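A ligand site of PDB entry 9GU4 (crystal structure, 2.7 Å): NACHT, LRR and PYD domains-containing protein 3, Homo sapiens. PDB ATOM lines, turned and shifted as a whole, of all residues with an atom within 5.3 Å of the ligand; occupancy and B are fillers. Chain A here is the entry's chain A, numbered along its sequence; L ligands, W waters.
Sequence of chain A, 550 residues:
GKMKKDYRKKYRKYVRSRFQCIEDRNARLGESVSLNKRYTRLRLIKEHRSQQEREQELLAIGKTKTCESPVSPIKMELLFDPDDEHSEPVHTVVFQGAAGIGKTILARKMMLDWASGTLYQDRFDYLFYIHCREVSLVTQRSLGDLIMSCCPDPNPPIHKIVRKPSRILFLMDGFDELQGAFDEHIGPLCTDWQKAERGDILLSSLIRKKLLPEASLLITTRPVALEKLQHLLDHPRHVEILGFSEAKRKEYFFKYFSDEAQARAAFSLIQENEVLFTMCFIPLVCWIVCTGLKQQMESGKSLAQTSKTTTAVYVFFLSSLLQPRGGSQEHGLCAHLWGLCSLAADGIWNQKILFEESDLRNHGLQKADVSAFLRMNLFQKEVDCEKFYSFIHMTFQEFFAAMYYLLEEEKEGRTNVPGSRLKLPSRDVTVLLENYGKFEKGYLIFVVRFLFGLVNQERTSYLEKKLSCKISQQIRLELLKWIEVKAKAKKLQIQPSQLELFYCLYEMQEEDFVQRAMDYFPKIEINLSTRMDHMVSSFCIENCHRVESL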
ATOM      1  N   ALA A  98      17.788 -24.758  11.542  1.00  0.00           N
ATOM      2  CA  ALA A  98      18.162 -23.406  11.950  1.00  0.00           C
ATOM      3  C   ALA A  98      17.497 -22.357  11.027  1.00  0.00           C
ATOM      4  O   ALA A  98      16.994 -22.710   9.941  1.00  0.00           O
ATOM      5  CB  ALA A  98      19.679 -23.275  11.910  1.00  0.00           C
ATOM      6  N   ALA A  99      17.459 -21.079  11.442  1.00  0.00           N
ATOM      7  CA  ALA A  99      16.832 -20.043  10.631  1.00  0.00           C
ATOM      8  C   ALA A  99      17.528 -19.928   9.267  1.00  0.00           C
ATOM      9  O   ALA A  99      18.748 -20.026   9.202  1.00  0.00           O
ATOM     10  CB  ALA A  99      16.900 -18.717  11.372  1.00  0.00           C
ATOM     11  N   GLY A 100      16.754 -19.873   8.194  1.00  0.00           N
ATOM     12  CA  GLY A 100      17.308 -19.799   6.861  1.00  0.00           C
ATOM     13  C   GLY A 100      17.791 -21.106   6.274  1.00  0.00           C
ATOM     14  O   GLY A 100      18.286 -21.134   5.151  1.00  0.00           O
ATOM     15  N   VAL A 224      14.668 -24.301  18.722  1.00  0.00           N
ATOM     16  CA  VAL A 224      14.271 -23.556  19.919  1.00  0.00           C
ATOM     17  C   VAL A 224      12.912 -23.998  20.415  1.00  0.00           C
ATOM     18  O   VAL A 224      12.759 -24.246  21.612  1.00  0.00           O
ATOM     19  CB  VAL A 224      14.326 -22.006  19.774  1.00  0.00           C
ATOM     20  CG1 VAL A 224      15.703 -21.463  20.098  1.00  0.00           C
ATOM     21  CG2 VAL A 224      13.862 -21.545  18.398  1.00  0.00           C
ATOM     22  N   MET A 279      29.708 -20.438   6.708  1.00  0.00           N
ATOM     23  CA  MET A 279      28.353 -19.913   6.827  1.00  0.00           C
ATOM     24  C   MET A 279      27.457 -20.337   5.680  1.00  0.00           C
ATOM     25  O   MET A 279      26.244 -20.434   5.873  1.00  0.00           O
ATOM     26  CB  MET A 279      28.352 -18.386   6.917  1.00  0.00           C
ATOM     27  CG  MET A 279      28.699 -17.876   8.292  1.00  0.00           C
ATOM     28  SD  MET A 279      28.490 -16.092   8.495  1.00  0.00           S
ATOM     29  CE  MET A 279      26.704 -15.977   8.551  1.00  0.00           C
ATOM     30  N   PHE A 281      26.680 -23.034   4.513  1.00  0.00           N
ATOM     31  CA  PHE A 281      25.913 -24.258   4.681  1.00  0.00           C
ATOM     32  C   PHE A 281      24.398 -23.875   4.798  1.00  0.00           C
ATOM     33  O   PHE A 281      23.534 -24.610   4.353  1.00  0.00           O
ATOM     34  CB  PHE A 281      26.424 -25.083   5.876  1.00  0.00           C
ATOM     35  CG  PHE A 281      25.809 -24.801   7.225  1.00  0.00           C
ATOM     36  CD1 PHE A 281      26.332 -23.822   8.054  1.00  0.00           C
ATOM     37  CD2 PHE A 281      24.711 -25.517   7.675  1.00  0.00           C
ATOM     38  CE1 PHE A 281      25.789 -23.586   9.303  1.00  0.00           C
ATOM     39  CE2 PHE A 281      24.154 -25.262   8.919  1.00  0.00           C
ATOM     40  CZ  PHE A 281      24.690 -24.299   9.723  1.00  0.00           C
ATOM     41  N   ILE A 282      24.095 -22.680   5.362  1.00  0.00           N
ATOM     42  CA  ILE A 282      22.753 -22.139   5.461  1.00  0.00           C
ATOM     43  C   ILE A 282      22.377 -21.584   4.101  1.00  0.00           C
ATOM     44  O   ILE A 282      23.006 -20.641   3.622  1.00  0.00           O
ATOM     45  CB  ILE A 282      22.729 -21.012   6.518  1.00  0.00           C
ATOM     46  CG1 ILE A 282      23.135 -21.522   7.895  1.00  0.00           C
ATOM     47  CG2 ILE A 282      21.381 -20.330   6.561  1.00  0.00           C
ATOM     48  CD1 ILE A 282      24.063 -20.577   8.613  1.00  0.00           C
ATOM     49  N   LEU A 284      20.109 -19.604   3.251  1.00  0.00           N
ATOM     50  CA  LEU A 284      19.794 -18.180   3.322  1.00  0.00           C
ATOM     51  C   LEU A 284      21.082 -17.367   3.153  1.00  0.00           C
ATOM     52  O   LEU A 284      21.086 -16.401   2.397  1.00  0.00           O
ATOM     53  CB  LEU A 284      19.081 -17.802   4.637  1.00  0.00           C
ATOM     54  CG  LEU A 284      18.778 -16.311   4.814  1.00  0.00           C
ATOM     55  CD1 LEU A 284      17.902 -15.766   3.712  1.00  0.00           C
ATOM     56  CD2 LEU A 284      18.161 -16.055   6.141  1.00  0.00           C
ATOM     57  N   VAL A 285      22.193 -17.792   3.800  1.00  0.00           N
ATOM     58  CA  VAL A 285      23.499 -17.136   3.662  1.00  0.00           C
ATOM     59  C   VAL A 285      23.939 -17.215   2.204  1.00  0.00           C
ATOM     60  O   VAL A 285      24.397 -16.214   1.660  1.00  0.00           O
ATOM     61  CB  VAL A 285      24.569 -17.684   4.640  1.00  0.00           C
ATOM     62  CG1 VAL A 285      25.941 -17.073   4.365  1.00  0.00           C
ATOM     63  CG2 VAL A 285      24.154 -17.445   6.079  1.00  0.00           C
ATOM     64  N   ILE A 288      21.874 -14.471   0.377  1.00  0.00           N
ATOM     65  CA  ILE A 288      22.306 -13.149   0.834  1.00  0.00           C
ATOM     66  C   ILE A 288      23.672 -12.789   0.213  1.00  0.00           C
ATOM     67  O   ILE A 288      23.835 -11.693  -0.342  1.00  0.00           O
ATOM     68  CB  ILE A 288      22.329 -13.114   2.392  1.00  0.00           C
ATOM     69  CG1 ILE A 288      20.905 -13.147   2.957  1.00  0.00           C
ATOM     70  CG2 ILE A 288      23.079 -11.899   2.898  1.00  0.00           C
ATOM     71  CD1 ILE A 288      20.828 -13.275   4.392  1.00  0.00           C
ATOM     72  N   THR A 310      27.890 -12.663  11.363  1.00  0.00           N
ATOM     73  CA  THR A 310      26.572 -12.632  10.735  1.00  0.00           C
ATOM     74  C   THR A 310      26.128 -11.171  10.576  1.00  0.00           C
ATOM     75  O   THR A 310      25.582 -10.823   9.529  1.00  0.00           O
ATOM     76  CB  THR A 310      25.561 -13.449  11.534  1.00  0.00           C
ATOM     77  OG1 THR A 310      26.090 -14.744  11.787  1.00  0.00           O
ATOM     78  CG2 THR A 310      24.216 -13.579  10.837  1.00  0.00           C
ATOM     79  N   TYR A 314      25.015  -9.222   7.096  1.00  0.00           N
ATOM     80  CA  TYR A 314      23.755  -8.491   6.970  1.00  0.00           C
ATOM     81  C   TYR A 314      23.965  -7.026   6.658  1.00  0.00           C
ATOM     82  O   TYR A 314      23.255  -6.466   5.836  1.00  0.00           O
ATOM     83  CB  TYR A 314      22.862  -8.695   8.211  1.00  0.00           C
ATOM     84  CG  TYR A 314      22.055  -9.979   8.132  1.00  0.00           C
ATOM     85  CD1 TYR A 314      22.658 -11.190   7.858  1.00  0.00           C
ATOM     86  CD2 TYR A 314      20.683  -9.967   8.342  1.00  0.00           C
ATOM     87  CE1 TYR A 314      21.924 -12.365   7.765  1.00  0.00           C
ATOM     88  CE2 TYR A 314      19.927 -11.134   8.240  1.00  0.00           C
ATOM     89  CZ  TYR A 314      20.552 -12.337   7.956  1.00  0.00           C
ATOM     90  OH  TYR A 314      19.812 -13.482   7.862  1.00  0.00           O
ATOM     91  N   THR A 395      14.980 -13.406  10.188  1.00  0.00           N
ATOM     92  CA  THR A 395      16.269 -12.878  10.614  1.00  0.00           C
ATOM     93  C   THR A 395      16.407 -11.389  10.270  1.00  0.00           C
ATOM     94  O   THR A 395      17.041 -10.658  11.017  1.00  0.00           O
ATOM     95  CB  THR A 395      17.423 -13.720  10.036  1.00  0.00           C
ATOM     96  OG1 THR A 395      17.326 -13.762   8.607  1.00  0.00           O
ATOM     97  CG2 THR A 395      17.472 -15.125  10.607  1.00  0.00           C
ATOM     98  N   ILE A 445      16.454 -14.642  19.483  1.00  0.00           N
ATOM     99  CA  ILE A 445      17.790 -15.172  19.221  1.00  0.00           C
ATOM    100  C   ILE A 445      18.641 -14.204  18.398  1.00  0.00           C
ATOM    101  O   ILE A 445      19.729 -13.810  18.852  1.00  0.00           O
ATOM    102  CB  ILE A 445      17.760 -16.583  18.594  1.00  0.00           C
ATOM    103  CG1 ILE A 445      16.895 -17.551  19.417  1.00  0.00           C
ATOM    104  CG2 ILE A 445      19.162 -17.119  18.395  1.00  0.00           C
ATOM    105  CD1 ILE A 445      17.289 -17.709  20.802  1.00  0.00           C
ATOM    106  N   PHE A 446      18.174 -13.821  17.209  1.00  0.00           N
ATOM    107  CA  PHE A 446      18.931 -12.899  16.365  1.00  0.00           C
ATOM    108  C   PHE A 446      18.801 -11.459  16.846  1.00  0.00           C
ATOM    109  O   PHE A 446      19.673 -10.672  16.542  1.00  0.00           O
ATOM    110  CB  PHE A 446      18.595 -13.068  14.869  1.00  0.00           C
ATOM    111  CG  PHE A 446      18.966 -14.420  14.341  1.00  0.00           C
ATOM    112  CD1 PHE A 446      18.139 -15.514  14.530  1.00  0.00           C
ATOM    113  CD2 PHE A 446      20.161 -14.624  13.676  1.00  0.00           C
ATOM    114  CE1 PHE A 446      18.493 -16.769  14.059  1.00  0.00           C
ATOM    115  CE2 PHE A 446      20.523 -15.878  13.212  1.00  0.00           C
ATOM    116  CZ  PHE A 446      19.682 -16.949  13.411  1.00  0.00           C
ATOM    117  N   ARG A 449      21.662 -11.603  19.281  1.00  0.00           N
ATOM    118  CA  ARG A 449      22.903 -11.801  18.518  1.00  0.00           C
ATOM    119  C   ARG A 449      23.301 -10.564  17.714  1.00  0.00           C
ATOM    120  O   ARG A 449      24.472 -10.197  17.733  1.00  0.00           O
ATOM    121  CB  ARG A 449      22.774 -12.985  17.554  1.00  0.00           C
ATOM    122  CG  ARG A 449      23.221 -14.316  18.119  1.00  0.00           C
ATOM    123  CD  ARG A 449      23.353 -15.315  17.004  1.00  0.00           C
ATOM    124  NE  ARG A 449      22.852 -16.636  17.380  1.00  0.00           N
ATOM    125  CZ  ARG A 449      22.781 -17.666  16.544  1.00  0.00           C
ATOM    126  NH1 ARG A 449      23.155 -17.542  15.280  1.00  0.00           N
ATOM    127  NH2 ARG A 449      22.314 -18.841  16.971  1.00  0.00           N
ATOM    128  N   PHE A 450      22.343  -9.925  17.029  1.00  0.00           N
ATOM    129  CA  PHE A 450      22.612  -8.736  16.228  1.00  0.00           C
ATOM    130  C   PHE A 450      22.923  -7.525  17.104  1.00  0.00           C
ATOM    131  O   PHE A 450      23.651  -6.649  16.653  1.00  0.00           O
ATOM    132  CB  PHE A 450      21.513  -8.446  15.206  1.00  0.00           C
ATOM    133  CG  PHE A 450      21.502  -9.362  14.003  1.00  0.00           C
ATOM    134  CD1 PHE A 450      22.680  -9.705  13.359  1.00  0.00           C
ATOM    135  CD2 PHE A 450      20.310  -9.851  13.490  1.00  0.00           C
ATOM    136  CE1 PHE A 450      22.660 -10.529  12.237  1.00  0.00           C
ATOM    137  CE2 PHE A 450      20.304 -10.675  12.367  1.00  0.00           C
ATOM    138  CZ  PHE A 450      21.476 -11.013  11.744  1.00  0.00           C
ATOM    139  N   SER A 497      22.088 -21.053  25.750  1.00  0.00           N
ATOM    140  CA  SER A 497      23.016 -22.132  26.114  1.00  0.00           C
ATOM    141  C   SER A 497      24.460 -21.583  26.135  1.00  0.00           C
ATOM    142  O   SER A 497      24.694 -20.427  25.745  1.00  0.00           O
ATOM    143  CB  SER A 497      22.900 -23.291  25.129  1.00  0.00           C
ATOM    144  OG  SER A 497      23.498 -23.005  23.867  1.00  0.00           O
ATOM    145  N   LEU A 499      26.976 -22.636  24.252  1.00  0.00           N
ATOM    146  CA  LEU A 499      27.315 -22.529  22.833  1.00  0.00           C
ATOM    147  C   LEU A 499      26.613 -21.347  22.193  1.00  0.00           C
ATOM    148  O   LEU A 499      27.207 -20.690  21.349  1.00  0.00           O
ATOM    149  CB  LEU A 499      26.958 -23.820  22.088  1.00  0.00           C
ATOM    150  CG  LEU A 499      27.306 -23.850  20.616  1.00  0.00           C
ATOM    151  CD1 LEU A 499      28.794 -23.761  20.405  1.00  0.00           C
ATOM    152  CD2 LEU A 499      26.791 -25.099  19.991  1.00  0.00           C
ATOM    153  N   GLU A 500      25.368 -21.054  22.590  1.00  0.00           N
ATOM    154  CA  GLU A 500      24.649 -19.894  22.065  1.00  0.00           C
ATOM    155  C   GLU A 500      25.329 -18.616  22.529  1.00  0.00           C
ATOM    156  O   GLU A 500      25.534 -17.708  21.713  1.00  0.00           O
ATOM    157  CB  GLU A 500      23.171 -19.900  22.488  1.00  0.00           C
ATOM    158  CG  GLU A 500      22.387 -18.670  22.079  1.00  0.00           C
ATOM    159  CD  GLU A 500      22.440 -18.334  20.609  1.00  0.00           C
ATOM    160  OE1 GLU A 500      22.506 -19.271  19.781  1.00  0.00           O
ATOM    161  OE2 GLU A 500      22.423 -17.128  20.276  1.00  0.00           O
ATOM    162  N   TYR A 503      28.024 -17.810  20.216  1.00  0.00           N
ATOM    163  CA  TYR A 503      27.555 -17.182  18.974  1.00  0.00           C
ATOM    164  C   TYR A 503      27.382 -15.678  19.215  1.00  0.00           C
ATOM    165  O   TYR A 503      27.688 -14.882  18.327  1.00  0.00           O
ATOM    166  CB  TYR A 503      26.226 -17.786  18.488  1.00  0.00           C
ATOM    167  CG  TYR A 503      26.376 -19.030  17.636  1.00  0.00           C
ATOM    168  CD1 TYR A 503      26.564 -20.271  18.212  1.00  0.00           C
ATOM    169  CD2 TYR A 503      26.269 -18.968  16.255  1.00  0.00           C
ATOM    170  CE1 TYR A 503      26.690 -21.422  17.440  1.00  0.00           C
ATOM    171  CE2 TYR A 503      26.410 -20.113  15.468  1.00  0.00           C
ATOM    172  CZ  TYR A 503      26.606 -21.336  16.074  1.00  0.00           C
ATOM    173  OH  TYR A 503      26.755 -22.463  15.318  1.00  0.00           O
ATOM    174  N   MET A 532      30.166 -24.613  11.976  1.00  0.00           N
ATOM    175  CA  MET A 532      29.841 -23.286  12.443  1.00  0.00           C
ATOM    176  C   MET A 532      30.068 -23.255  13.956  1.00  0.00           C
ATOM    177  O   MET A 532      30.726 -22.356  14.471  1.00  0.00           O
ATOM    178  CB  MET A 532      28.378 -22.972  12.079  1.00  0.00           C
ATOM    179  CG  MET A 532      27.990 -21.549  12.306  1.00  0.00           C
ATOM    180  SD  MET A 532      28.916 -20.396  11.281  1.00  0.00           S
ATOM    181  CE  MET A 532      28.626 -18.881  12.181  1.00  0.00           C
ATOM    182  N   ASP A 533      29.573 -24.287  14.670  1.00  0.00           N
ATOM    183  CA  ASP A 533      29.749 -24.479  16.109  1.00  0.00           C
ATOM    184  C   ASP A 533      31.233 -24.522  16.449  1.00  0.00           C
ATOM    185  O   ASP A 533      31.624 -24.023  17.490  1.00  0.00           O
ATOM    186  CB  ASP A 533      29.123 -25.803  16.550  1.00  0.00           C
ATOM    187  CG  ASP A 533      27.618 -25.831  16.630  1.00  0.00           C
ATOM    188  OD1 ASP A 533      27.001 -24.763  16.451  1.00  0.00           O
ATOM    189  OD2 ASP A 533      27.055 -26.913  16.884  1.00  0.00           O
HETATM  190  C1  LIG L   1      22.797 -20.329  12.863  1.00  0.00           C
HETATM  191  C2  LIG L   1      22.602 -19.277  11.854  1.00  0.00           C
HETATM  192  C3  LIG L   1      23.619 -18.377  11.559  1.00  0.00           C
HETATM  193  C4  LIG L   1      23.105 -22.106  14.943  1.00  0.00           C
HETATM  194  C5  LIG L   1      23.336 -22.527  13.630  1.00  0.00           C
HETATM  195  C6  LIG L   1      23.185 -21.632  12.578  1.00  0.00           C
HETATM  196  C7  LIG L   1      23.092 -22.312  17.400  1.00  0.00           C
HETATM  197  C8  LIG L   1      21.603 -22.132  17.778  1.00  0.00           C
HETATM  198  C9  LIG L   1      22.033 -22.529  20.117  1.00  0.00           C
HETATM  199  C10 LIG L   1      23.533 -22.735  19.840  1.00  0.00           C
HETATM  200  C11 LIG L   1      23.728 -23.286  18.415  1.00  0.00           C
HETATM  201  C12 LIG L   1      20.089 -21.116  19.415  1.00  0.00           C
HETATM  202  C13 LIG L   1      19.114 -22.308  19.489  1.00  0.00           C
HETATM  203  C14 LIG L   1      21.921 -16.184   8.948  1.00  0.00           C
HETATM  204  C15 LIG L   1      23.389 -17.384  10.602  1.00  0.00           C
HETATM  205  C16 LIG L   1      22.151 -17.293   9.977  1.00  0.00           C
HETATM  206  C17 LIG L   1      21.142 -18.187  10.292  1.00  0.00           C
HETATM  207  C18 LIG L   1      21.365 -19.172  11.240  1.00  0.00           C
HETATM  208  O1  LIG L   1      20.370 -20.083  11.574  1.00  0.00           O
HETATM  209  C19 LIG L   1      24.993 -18.461  12.227  1.00  0.00           C
HETATM  210  N1  LIG L   1      22.591 -19.980  14.135  1.00  0.00           N
HETATM  211  N2  LIG L   1      22.734 -20.835  15.141  1.00  0.00           N
HETATM  212  N3  LIG L   1      23.212 -22.862  16.058  1.00  0.00           N
HETATM  213  N4  LIG L   1      21.469 -21.578  19.134  1.00  0.00           N
HETATM  214  F1  LIG L   1      21.001 -16.538   8.040  1.00  0.00           F
HETATM  215  F2  LIG L   1      21.492 -15.088   9.600  1.00  0.00           F
HETATM  216  F3  LIG L   1      23.073 -15.893   8.323  1.00  0.00           F
HETATM  217  O   HOH W   1      24.924 -15.617  14.138  1.00  0.00           O
HETATM  218  O   HOH W   2      17.248 -22.733  16.817  1.00  0.00           O
HETATM  219  O   HOH W   3      18.981 -21.042  14.480  1.00  0.00           O
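Water W3 bridges O1 of the ligand (3.4 Å) and N of Ala 99 (3.4 Å). Water W1 bridges OG1 of Thr 310 (2.8 Å) and NH1 of Arg 449 (2.9 Å).
A fluorine (F2) of the ligand lies close to the side-chain hydroxyl of Tyr 314 (2.9 Å). Ala 98 touches the ligand (CB to O1, 3.3 Å). CG1 of Val 224 touches C13 of the ligand (3.6 Å). CE of Met 279 touches F3 of the ligand, at 3.6 Å. Ile 282 touches the ligand (CD1 to C3, 3.7 Å). Leu 284 touches the ligand. CG2 of Val 285 touches F3 of the ligand, at 2.9 Å. CG2 of Thr 310 touches F2 of the ligand, at 3.4 Å. Phe 446 touches the ligand. Leu 499 touches the ligand (CD2 to C11, 3.9 Å). Tyr 503 touches the ligand. CE of Met 532 touches C19 of the ligand, 3.7 Å away. Within 4 Å of the ligand: Ala 98, Ala 99, Val 224, Met 279, Ile 282, Leu 284, Val 285, Thr 310, Tyr 314, Phe 446, Arg 449, Leu 499, Glu 500, Tyr 503 and Met 532.
The guanidinium group of Arg 449 is in salt-bridge range of the side-chain carboxylate of Glu 500 (2.8 Å). OH of Tyr 503 is in hydrogen-bond range of OD1 of Asp 533. OG of Ser 497 lies within hydrogen-bond range of N of Glu 500 (3.0 Å). OH of Tyr 314 lies within hydrogen-bond range of OG1 of Thr 395 (2.6 Å). The backbone NH of Leu 284 is in hydrogen-bond range of the backbone carbonyl oxygen of Gly 100 (3.0 Å).
NH2 of Arg 449 lies within hydrogen-bond range of N2 of the ligand (2.7 Å). O1 of the ligand is in hydrogen-bond range of O of Ala 99 (2.9 Å). The side-chain carboxylate of Glu 500 is in salt-bridge range of a nitrogen (N4) of the ligand. The backbone NH (N) of Ala 99 lies within hydrogen-bond range of an oxygen (O1) of the ligand (3.1 Å).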
